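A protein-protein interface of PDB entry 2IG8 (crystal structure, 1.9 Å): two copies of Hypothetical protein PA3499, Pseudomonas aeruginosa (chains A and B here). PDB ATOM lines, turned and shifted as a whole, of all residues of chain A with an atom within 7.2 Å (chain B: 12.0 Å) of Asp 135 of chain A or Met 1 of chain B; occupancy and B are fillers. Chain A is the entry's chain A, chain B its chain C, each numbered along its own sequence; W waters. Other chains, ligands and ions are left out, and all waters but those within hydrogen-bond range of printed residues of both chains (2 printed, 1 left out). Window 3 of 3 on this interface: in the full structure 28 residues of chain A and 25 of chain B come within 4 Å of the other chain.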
ATOM      1  N   GLU A  28     -27.120   4.349  -6.690  1.00  0.00           N
ATOM      2  CA  GLU A  28     -26.724   3.696  -5.441  1.00  0.00           C
ATOM      3  C   GLU A  28     -25.411   4.290  -4.857  1.00  0.00           C
ATOM      4  O   GLU A  28     -24.976   3.898  -3.785  1.00  0.00           O
ATOM      5  CB  GLU A  28     -26.651   2.186  -5.638  1.00  0.00           C
ATOM      6  CG  GLU A  28     -27.304   1.346  -4.510  1.00  0.00           C
ATOM      7  CD  GLU A  28     -28.858   1.366  -4.445  1.00  0.00           C
ATOM      8  OE1 GLU A  28     -29.413   0.519  -3.708  1.00  0.00           O
ATOM      9  OE2 GLU A  28     -29.527   2.219  -5.085  1.00  0.00           O
ATOM     10  N   GLU A  29     -24.801   5.255  -5.541  1.00  0.00           N
ATOM     11  CA  GLU A  29     -23.568   5.882  -5.045  1.00  0.00           C
ATOM     12  C   GLU A  29     -23.856   7.026  -4.081  1.00  0.00           C
ATOM     13  O   GLU A  29     -24.606   7.947  -4.418  1.00  0.00           O
ATOM     14  CB  GLU A  29     -22.723   6.404  -6.221  1.00  0.00           C
ATOM     15  CG  GLU A  29     -21.343   6.972  -5.806  1.00  0.00           C
ATOM     16  CD  GLU A  29     -20.207   5.911  -5.806  1.00  0.00           C
ATOM     17  OE1 GLU A  29     -20.397   4.803  -6.331  1.00  0.00           O
ATOM     18  OE2 GLU A  29     -19.118   6.201  -5.268  1.00  0.00           O
ATOM     19  N   ASN A  77     -20.695   0.226   3.547  1.00  0.00           N
ATOM     20  CA  ASN A  77     -20.877   0.749   2.183  1.00  0.00           C
ATOM     21  C   ASN A  77     -19.648   1.472   1.636  1.00  0.00           C
ATOM     22  O   ASN A  77     -19.551   1.723   0.429  1.00  0.00           O
ATOM     23  CB  ASN A  77     -22.042   1.741   2.139  1.00  0.00           C
ATOM     24  CG  ASN A  77     -23.387   1.113   2.476  1.00  0.00           C
ATOM     25  OD1 ASN A  77     -23.612  -0.091   2.325  1.00  0.00           O
ATOM     26  ND2 ASN A  77     -24.293   1.946   2.923  1.00  0.00           N
ATOM     27  N   ALA A 132     -18.602   5.731  -1.205  1.00  0.00           N
ATOM     28  CA  ALA A 132     -19.474   4.684  -0.732  1.00  0.00           C
ATOM     29  C   ALA A 132     -20.609   4.363  -1.707  1.00  0.00           C
ATOM     30  O   ALA A 132     -21.033   5.203  -2.516  1.00  0.00           O
ATOM     31  CB  ALA A 132     -20.035   5.074   0.614  1.00  0.00           C
ATOM     32  N   ARG A 133     -21.092   3.132  -1.593  1.00  0.00           N
ATOM     33  CA  ARG A 133     -22.177   2.590  -2.401  1.00  0.00           C
ATOM     34  C   ARG A 133     -23.153   1.850  -1.509  1.00  0.00           C
ATOM     35  O   ARG A 133     -22.729   0.996  -0.748  1.00  0.00           O
ATOM     36  CB  ARG A 133     -21.601   1.570  -3.348  1.00  0.00           C
ATOM     37  CG  ARG A 133     -21.344   2.085  -4.664  1.00  0.00           C
ATOM     38  CD  ARG A 133     -20.711   1.016  -5.461  1.00  0.00           C
ATOM     39  NE  ARG A 133     -21.672   0.185  -6.163  1.00  0.00           N
ATOM     40  CZ  ARG A 133     -21.436  -0.319  -7.371  1.00  0.00           C
ATOM     41  NH1 ARG A 133     -20.304  -0.024  -8.022  1.00  0.00           N
ATOM     42  NH2 ARG A 133     -22.338  -1.086  -7.960  1.00  0.00           N
ATOM     43  N   LEU A 134     -24.452   2.132  -1.625  1.00  0.00           N
ATOM     44  CA  LEU A 134     -25.439   1.508  -0.743  1.00  0.00           C
ATOM     45  C   LEU A 134     -25.745   0.035  -1.063  1.00  0.00           C
ATOM     46  O   LEU A 134     -26.376  -0.642  -0.261  1.00  0.00           O
ATOM     47  CB  LEU A 134     -26.748   2.327  -0.688  1.00  0.00           C
ATOM     48  CG  LEU A 134     -26.654   3.757  -0.131  1.00  0.00           C
ATOM     49  CD1 LEU A 134     -28.049   4.347   0.042  1.00  0.00           C
ATOM     50  CD2 LEU A 134     -25.898   3.815   1.190  1.00  0.00           C
ATOM     51  N   ASP A 135     -25.271  -0.471  -2.200  1.00  0.00           N
ATOM     52  CA  ASP A 135     -25.564  -1.846  -2.594  1.00  0.00           C
ATOM     53  C   ASP A 135     -24.443  -2.853  -2.264  1.00  0.00           C
ATOM     54  O   ASP A 135     -24.526  -4.003  -2.649  1.00  0.00           O
ATOM     55  CB  ASP A 135     -25.902  -1.908  -4.088  1.00  0.00           C
ATOM     56  CG  ASP A 135     -24.821  -1.355  -4.962  1.00  0.00           C
ATOM     57  OD1 ASP A 135     -23.951  -0.583  -4.479  1.00  0.00           O
ATOM     58  OD2 ASP A 135     -24.852  -1.682  -6.161  1.00  0.00           O
ATOM     59  N   ILE A 136     -23.406  -2.416  -1.556  1.00  0.00           N
ATOM     60  CA  ILE A 136     -22.351  -3.308  -1.119  1.00  0.00           C
ATOM     61  C   ILE A 136     -22.241  -3.282   0.393  1.00  0.00           C
ATOM     62  O   ILE A 136     -22.720  -2.356   1.048  1.00  0.00           O
ATOM     63  CB  ILE A 136     -20.977  -2.913  -1.712  1.00  0.00           C
ATOM     64  CG1 ILE A 136     -20.453  -1.622  -1.065  1.00  0.00           C
ATOM     65  CG2 ILE A 136     -21.067  -2.771  -3.230  1.00  0.00           C
ATOM     66  CD1 ILE A 136     -19.094  -1.152  -1.626  1.00  0.00           C
ATOM     67  N   ASP A 137     -21.594  -4.309   0.926  1.00  0.00           N
ATOM     68  CA  ASP A 137     -21.208  -4.368   2.320  1.00  0.00           C
ATOM     69  C   ASP A 137     -19.867  -5.080   2.412  1.00  0.00           C
ATOM     70  O   ASP A 137     -19.793  -6.298   2.154  1.00  0.00           O
ATOM     71  CB  ASP A 137     -22.268  -5.130   3.123  1.00  0.00           C
ATOM     72  CG  ASP A 137     -21.996  -5.126   4.621  1.00  0.00           C
ATOM     73  OD1 ASP A 137     -20.935  -4.623   5.035  1.00  0.00           O
ATOM     74  OD2 ASP A 137     -22.857  -5.610   5.386  1.00  0.00           O
ATOM     75  N   LEU A 138     -18.821  -4.338   2.792  1.00  0.00           N
ATOM     76  CA  LEU A 138     -17.474  -4.898   2.889  1.00  0.00           C
ATOM     77  C   LEU A 138     -17.387  -5.941   3.986  1.00  0.00           C
ATOM     78  O   LEU A 138     -16.453  -6.731   3.993  1.00  0.00           O
ATOM     79  CB  LEU A 138     -16.397  -3.820   3.107  1.00  0.00           C
ATOM     80  CG  LEU A 138     -15.766  -3.250   1.834  1.00  0.00           C
ATOM     81  CD1 LEU A 138     -16.823  -2.638   0.956  1.00  0.00           C
ATOM     82  CD2 LEU A 138     -14.658  -2.256   2.170  1.00  0.00           C
ATOM     83  N   ASN A 140     -19.245  -8.385   3.996  1.00  0.00           N
ATOM     84  CA  ASN A 140     -19.495  -9.568   3.167  1.00  0.00           C
ATOM     85  C   ASN A 140     -18.486  -9.738   2.038  1.00  0.00           C
ATOM     86  O   ASN A 140     -18.793 -10.298   0.979  1.00  0.00           O
ATOM     87  CB  ASN A 140     -20.881  -9.462   2.557  1.00  0.00           C
ATOM     88  CG  ASN A 140     -21.949  -9.471   3.596  1.00  0.00           C
ATOM     89  OD1 ASN A 140     -21.822 -10.152   4.616  1.00  0.00           O
ATOM     90  ND2 ASN A 140     -23.009  -8.729   3.356  1.00  0.00           N
ATOM     91  N   MET B   1     -28.065  -5.908  -4.656  1.00  0.00           N
ATOM     92  CA  MET B   1     -26.732  -6.036  -4.010  1.00  0.00           C
ATOM     93  C   MET B   1     -25.659  -6.378  -5.025  1.00  0.00           C
ATOM     94  O   MET B   1     -25.875  -7.171  -5.951  1.00  0.00           O
ATOM     95  CB  MET B   1     -26.727  -7.101  -2.908  1.00  0.00           C
ATOM     96  CG  MET B   1     -25.328  -7.289  -2.282  1.00  0.00           C
ATOM     97  SD  MET B   1     -25.317  -7.924  -0.593  1.00  0.00           S
ATOM     98  CE  MET B   1     -23.852  -7.120   0.086  1.00  0.00           C
ATOM     99  N   THR B   2     -24.494  -5.785  -4.805  1.00  0.00           N
ATOM    100  CA  THR B   2     -23.345  -5.953  -5.662  1.00  0.00           C
ATOM    101  C   THR B   2     -22.252  -6.622  -4.854  1.00  0.00           C
ATOM    102  O   THR B   2     -22.013  -6.280  -3.688  1.00  0.00           O
ATOM    103  CB  THR B   2     -22.884  -4.607  -6.189  1.00  0.00           C
ATOM    104  OG1 THR B   2     -23.944  -4.034  -6.960  1.00  0.00           O
ATOM    105  CG2 THR B   2     -21.629  -4.747  -7.056  1.00  0.00           C
ATOM    106  N   ALA B   3     -21.618  -7.613  -5.489  1.00  0.00           N
ATOM    107  CA  ALA B   3     -20.592  -8.428  -4.858  1.00  0.00           C
ATOM    108  C   ALA B   3     -19.328  -7.621  -4.711  1.00  0.00           C
ATOM    109  O   ALA B   3     -18.983  -6.839  -5.608  1.00  0.00           O
ATOM    110  CB  ALA B   3     -20.321  -9.678  -5.695  1.00  0.00           C
ATOM    111  N   VAL B   4     -18.657  -7.765  -3.574  1.00  0.00           N
ATOM    112  CA  VAL B   4     -17.317  -7.217  -3.421  1.00  0.00           C
ATOM    113  C   VAL B   4     -16.386  -8.397  -3.162  1.00  0.00           C
ATOM    114  O   VAL B   4     -16.652  -9.243  -2.302  1.00  0.00           O
ATOM    115  CB  VAL B   4     -17.206  -6.117  -2.334  1.00  0.00           C
ATOM    116  CG1 VAL B   4     -18.375  -5.135  -2.447  1.00  0.00           C
ATOM    117  CG2 VAL B   4     -17.185  -6.694  -0.949  1.00  0.00           C
ATOM    118  N   ARG B   5     -15.330  -8.478  -3.958  1.00  0.00           N
ATOM    119  CA  ARG B   5     -14.323  -9.525  -3.794  1.00  0.00           C
ATOM    120  C   ARG B   5     -13.021  -8.811  -3.545  1.00  0.00           C
ATOM    121  O   ARG B   5     -12.681  -7.853  -4.267  1.00  0.00           O
ATOM    122  CB  ARG B   5     -14.226 -10.403  -5.037  1.00  0.00           C
ATOM    123  CG  ARG B   5     -13.099 -11.442  -4.945  1.00  0.00           C
ATOM    124  CD  ARG B   5     -13.292 -12.625  -5.878  1.00  0.00           C
ATOM    125  NE  ARG B   5     -12.368 -12.597  -7.015  1.00  0.00           N
ATOM    126  CZ  ARG B   5     -12.659 -12.156  -8.243  1.00  0.00           C
ATOM    127  NH1 ARG B   5     -13.876 -11.703  -8.548  1.00  0.00           N
ATOM    128  NH2 ARG B   5     -11.720 -12.184  -9.185  1.00  0.00           N
ATOM    129  N   LEU B  25     -12.700  -5.602  -5.829  1.00  0.00           N
ATOM    130  CA  LEU B  25     -13.510  -5.650  -7.033  1.00  0.00           C
ATOM    131  C   LEU B  25     -14.950  -5.479  -6.605  1.00  0.00           C
ATOM    132  O   LEU B  25     -15.507  -6.343  -5.930  1.00  0.00           O
ATOM    133  CB  LEU B  25     -13.331  -6.963  -7.786  1.00  0.00           C
ATOM    134  CG  LEU B  25     -14.073  -7.063  -9.128  1.00  0.00           C
ATOM    135  CD1 LEU B  25     -13.626  -5.970 -10.113  1.00  0.00           C
ATOM    136  CD2 LEU B  25     -13.855  -8.464  -9.711  1.00  0.00           C
ATOM    137  N   VAL B  26     -15.527  -4.342  -6.979  1.00  0.00           N
ATOM    138  CA  VAL B  26     -16.872  -3.972  -6.579  1.00  0.00           C
ATOM    139  C   VAL B  26     -17.669  -3.984  -7.879  1.00  0.00           C
ATOM    140  O   VAL B  26     -17.592  -3.033  -8.678  1.00  0.00           O
ATOM    141  CB  VAL B  26     -16.858  -2.584  -5.925  1.00  0.00           C
ATOM    142  CG1 VAL B  26     -18.232  -2.194  -5.458  1.00  0.00           C
ATOM    143  CG2 VAL B  26     -15.850  -2.549  -4.770  1.00  0.00           C
ATOM    144  N   GLY B  27     -18.391  -5.073  -8.114  1.00  0.00           N
ATOM    145  CA  GLY B  27     -19.020  -5.319  -9.413  1.00  0.00           C
ATOM    146  C   GLY B  27     -17.977  -5.410 -10.524  1.00  0.00           C
ATOM    147  O   GLY B  27     -17.135  -6.310 -10.507  1.00  0.00           O
ATOM    148  N   GLU B  28     -18.022  -4.464 -11.474  1.00  0.00           N
ATOM    149  CA  GLU B  28     -17.050  -4.408 -12.561  1.00  0.00           C
ATOM    150  C   GLU B  28     -15.927  -3.429 -12.230  1.00  0.00           C
ATOM    151  O   GLU B  28     -14.898  -3.403 -12.917  1.00  0.00           O
ATOM    152  CB  GLU B  28     -17.715  -3.998 -13.884  1.00  0.00           C
ATOM    153  CG  GLU B  28     -18.773  -4.973 -14.415  1.00  0.00           C
ATOM    154  CD  GLU B  28     -18.209  -6.237 -15.075  1.00  0.00           C
ATOM    155  OE1 GLU B  28     -16.972  -6.358 -15.255  1.00  0.00           O
ATOM    156  OE2 GLU B  28     -19.023  -7.122 -15.431  1.00  0.00           O
ATOM    157  N   GLU B  29     -16.114  -2.657 -11.166  1.00  0.00           N
ATOM    158  CA  GLU B  29     -15.188  -1.601 -10.796  1.00  0.00           C
ATOM    159  C   GLU B  29     -14.049  -2.176  -9.966  1.00  0.00           C
ATOM    160  O   GLU B  29     -14.298  -2.789  -8.946  1.00  0.00           O
ATOM    161  CB  GLU B  29     -15.921  -0.506 -10.000  1.00  0.00           C
ATOM    162  CG  GLU B  29     -15.055   0.677  -9.621  1.00  0.00           C
ATOM    163  CD  GLU B  29     -14.884   1.696 -10.755  1.00  0.00           C
ATOM    164  OE1 GLU B  29     -15.718   1.711 -11.687  1.00  0.00           O
ATOM    165  OE2 GLU B  29     -13.925   2.494 -10.702  1.00  0.00           O
ATOM    166  N   VAL B  31     -11.478  -1.179  -7.544  1.00  0.00           N
ATOM    167  CA  VAL B  31     -11.160  -0.050  -6.665  1.00  0.00           C
ATOM    168  C   VAL B  31      -9.765  -0.335  -6.134  1.00  0.00           C
ATOM    169  O   VAL B  31      -9.513  -1.431  -5.654  1.00  0.00           O
ATOM    170  CB  VAL B  31     -12.155   0.059  -5.506  1.00  0.00           C
ATOM    171  CG1 VAL B  31     -11.806   1.238  -4.599  1.00  0.00           C
ATOM    172  CG2 VAL B  31     -13.586   0.210  -6.041  1.00  0.00           C
ATOM    173  N   ARG B 133     -12.283  -0.227 -14.635  1.00  0.00           N
ATOM    174  CA  ARG B 133     -13.347  -1.198 -14.628  1.00  0.00           C
ATOM    175  C   ARG B 133     -13.160  -2.258 -15.689  1.00  0.00           C
ATOM    176  O   ARG B 133     -12.663  -2.005 -16.797  1.00  0.00           O
ATOM    177  CB  ARG B 133     -14.703  -0.523 -14.752  1.00  0.00           C
ATOM    178  CG  ARG B 133     -14.892   0.309 -16.000  1.00  0.00           C
ATOM    179  CD  ARG B 133     -16.074   1.226 -15.825  1.00  0.00           C
ATOM    180  NE  ARG B 133     -17.172   0.559 -15.123  1.00  0.00           N
ATOM    181  CZ  ARG B 133     -18.398   0.354 -15.611  1.00  0.00           C
ATOM    182  NH1 ARG B 133     -19.310  -0.257 -14.854  1.00  0.00           N
ATOM    183  NH2 ARG B 133     -18.733   0.751 -16.840  1.00  0.00           N
HETATM  184  O   HOH W   1     -19.825  -8.989  -1.022  1.00  0.00           O
HETATM  185  O   HOH W   2     -21.372  -6.603  -1.101  1.00  0.00           O
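OG1 of Thr 2 of chain B lies within hydrogen-bond range of OD2 of Asp 135 of chain A, at 2.6 Å.
Positions printed for both chains: 28, 29 and 133. Of the 9 pairs that touch across the chains among the printed residues, none has its exchanged pair printed and touching as well.
Among the printed residues, no Asp or Glu carboxylate lies within 4 Å of a Lys or Arg side-chain nitrogen of the other chain.
Water W1 lies within hydrogen-bond range of O of Asn 140 of chain A (2.6 Å) and N of Val 4 of chain B (3.1 Å). Water W2 bridges O of Thr 2 of chain B (2.7 Å) and N of Asp 137 of chain A (3.1 Å).
N of Arg 133 of chain A sits at hydrogen-bond distance from O of Asn 77 of chain A, at 2.9 Å. OD1 of Asn 77 of chain A sits close to O of Ile 136 of chain A (2.7 Å). The guanidinium group (NE) of Arg 133 of chain A is in salt-bridge range of the side-chain carboxylate (OD1) of Asp 135 of chain A (2.9 Å).
Among the printed residues, pairs that only touch across the chains: Arg 133 of chain A with Thr 2 of chain B (3.5 Å), Arg 133 of chain A with Val 26 of chain B (3.9 Å), Asp 135 of chain A with Met 1 of chain B (3.3 Å), Ile 136 of chain A with Thr 2 of chain B (3.7 Å), Ile 136 of chain A with Val 4 of chain B (3.5 Å), Ile 136 of chain A with Val 26 of chain B (3.7 Å), Asp 137 of chain A with Met 1 of chain B (3.7 Å) and Asn 140 of chain A with Met 1 of chain B (3.7 Å).
Of chain B, only Met 1 and Thr 2 come within 4 Å of Asp 135 of chain A. Met 1 of chain B touches just these residues of chain A: Asp 135, Asp 137 and Asn 140. No residue of chain B comes within 4 Å of Glu 28 of chain A. No residue of chain B comes within 4 Å of Asn 77 of chain A. No residue of chain B comes within 4 Å of Leu 134 of chain A. Of chain B, only Thr 2, Val 4 and Val 26 come within 4 Å of Ile 136 of chain A. Asp 137 of chain A touches one residue of chain B. Asn 140 of chain A touches just one residue of chain B: Met 1 (3.7 Å). Of the printed residues of chain A, Thr 2 of chain B touches Arg 133, Asp 135 and Ile 136. Printed residues of chain A within 4 Å of Val 26 of chain B: Arg 133 (3.9 Å) and Ile 136 (3.7 Å). Printed residues of chain A within 4 Å of Val 4 of chain B: Ile 136. The nearest residue of chain B that does not touch Asp 135 of chain A is Ala 3 of chain B (5.4 Å). The nearest residue of chain A that does not touch Met 1 of chain B is Ile 136 of chain A (4.2 Å).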
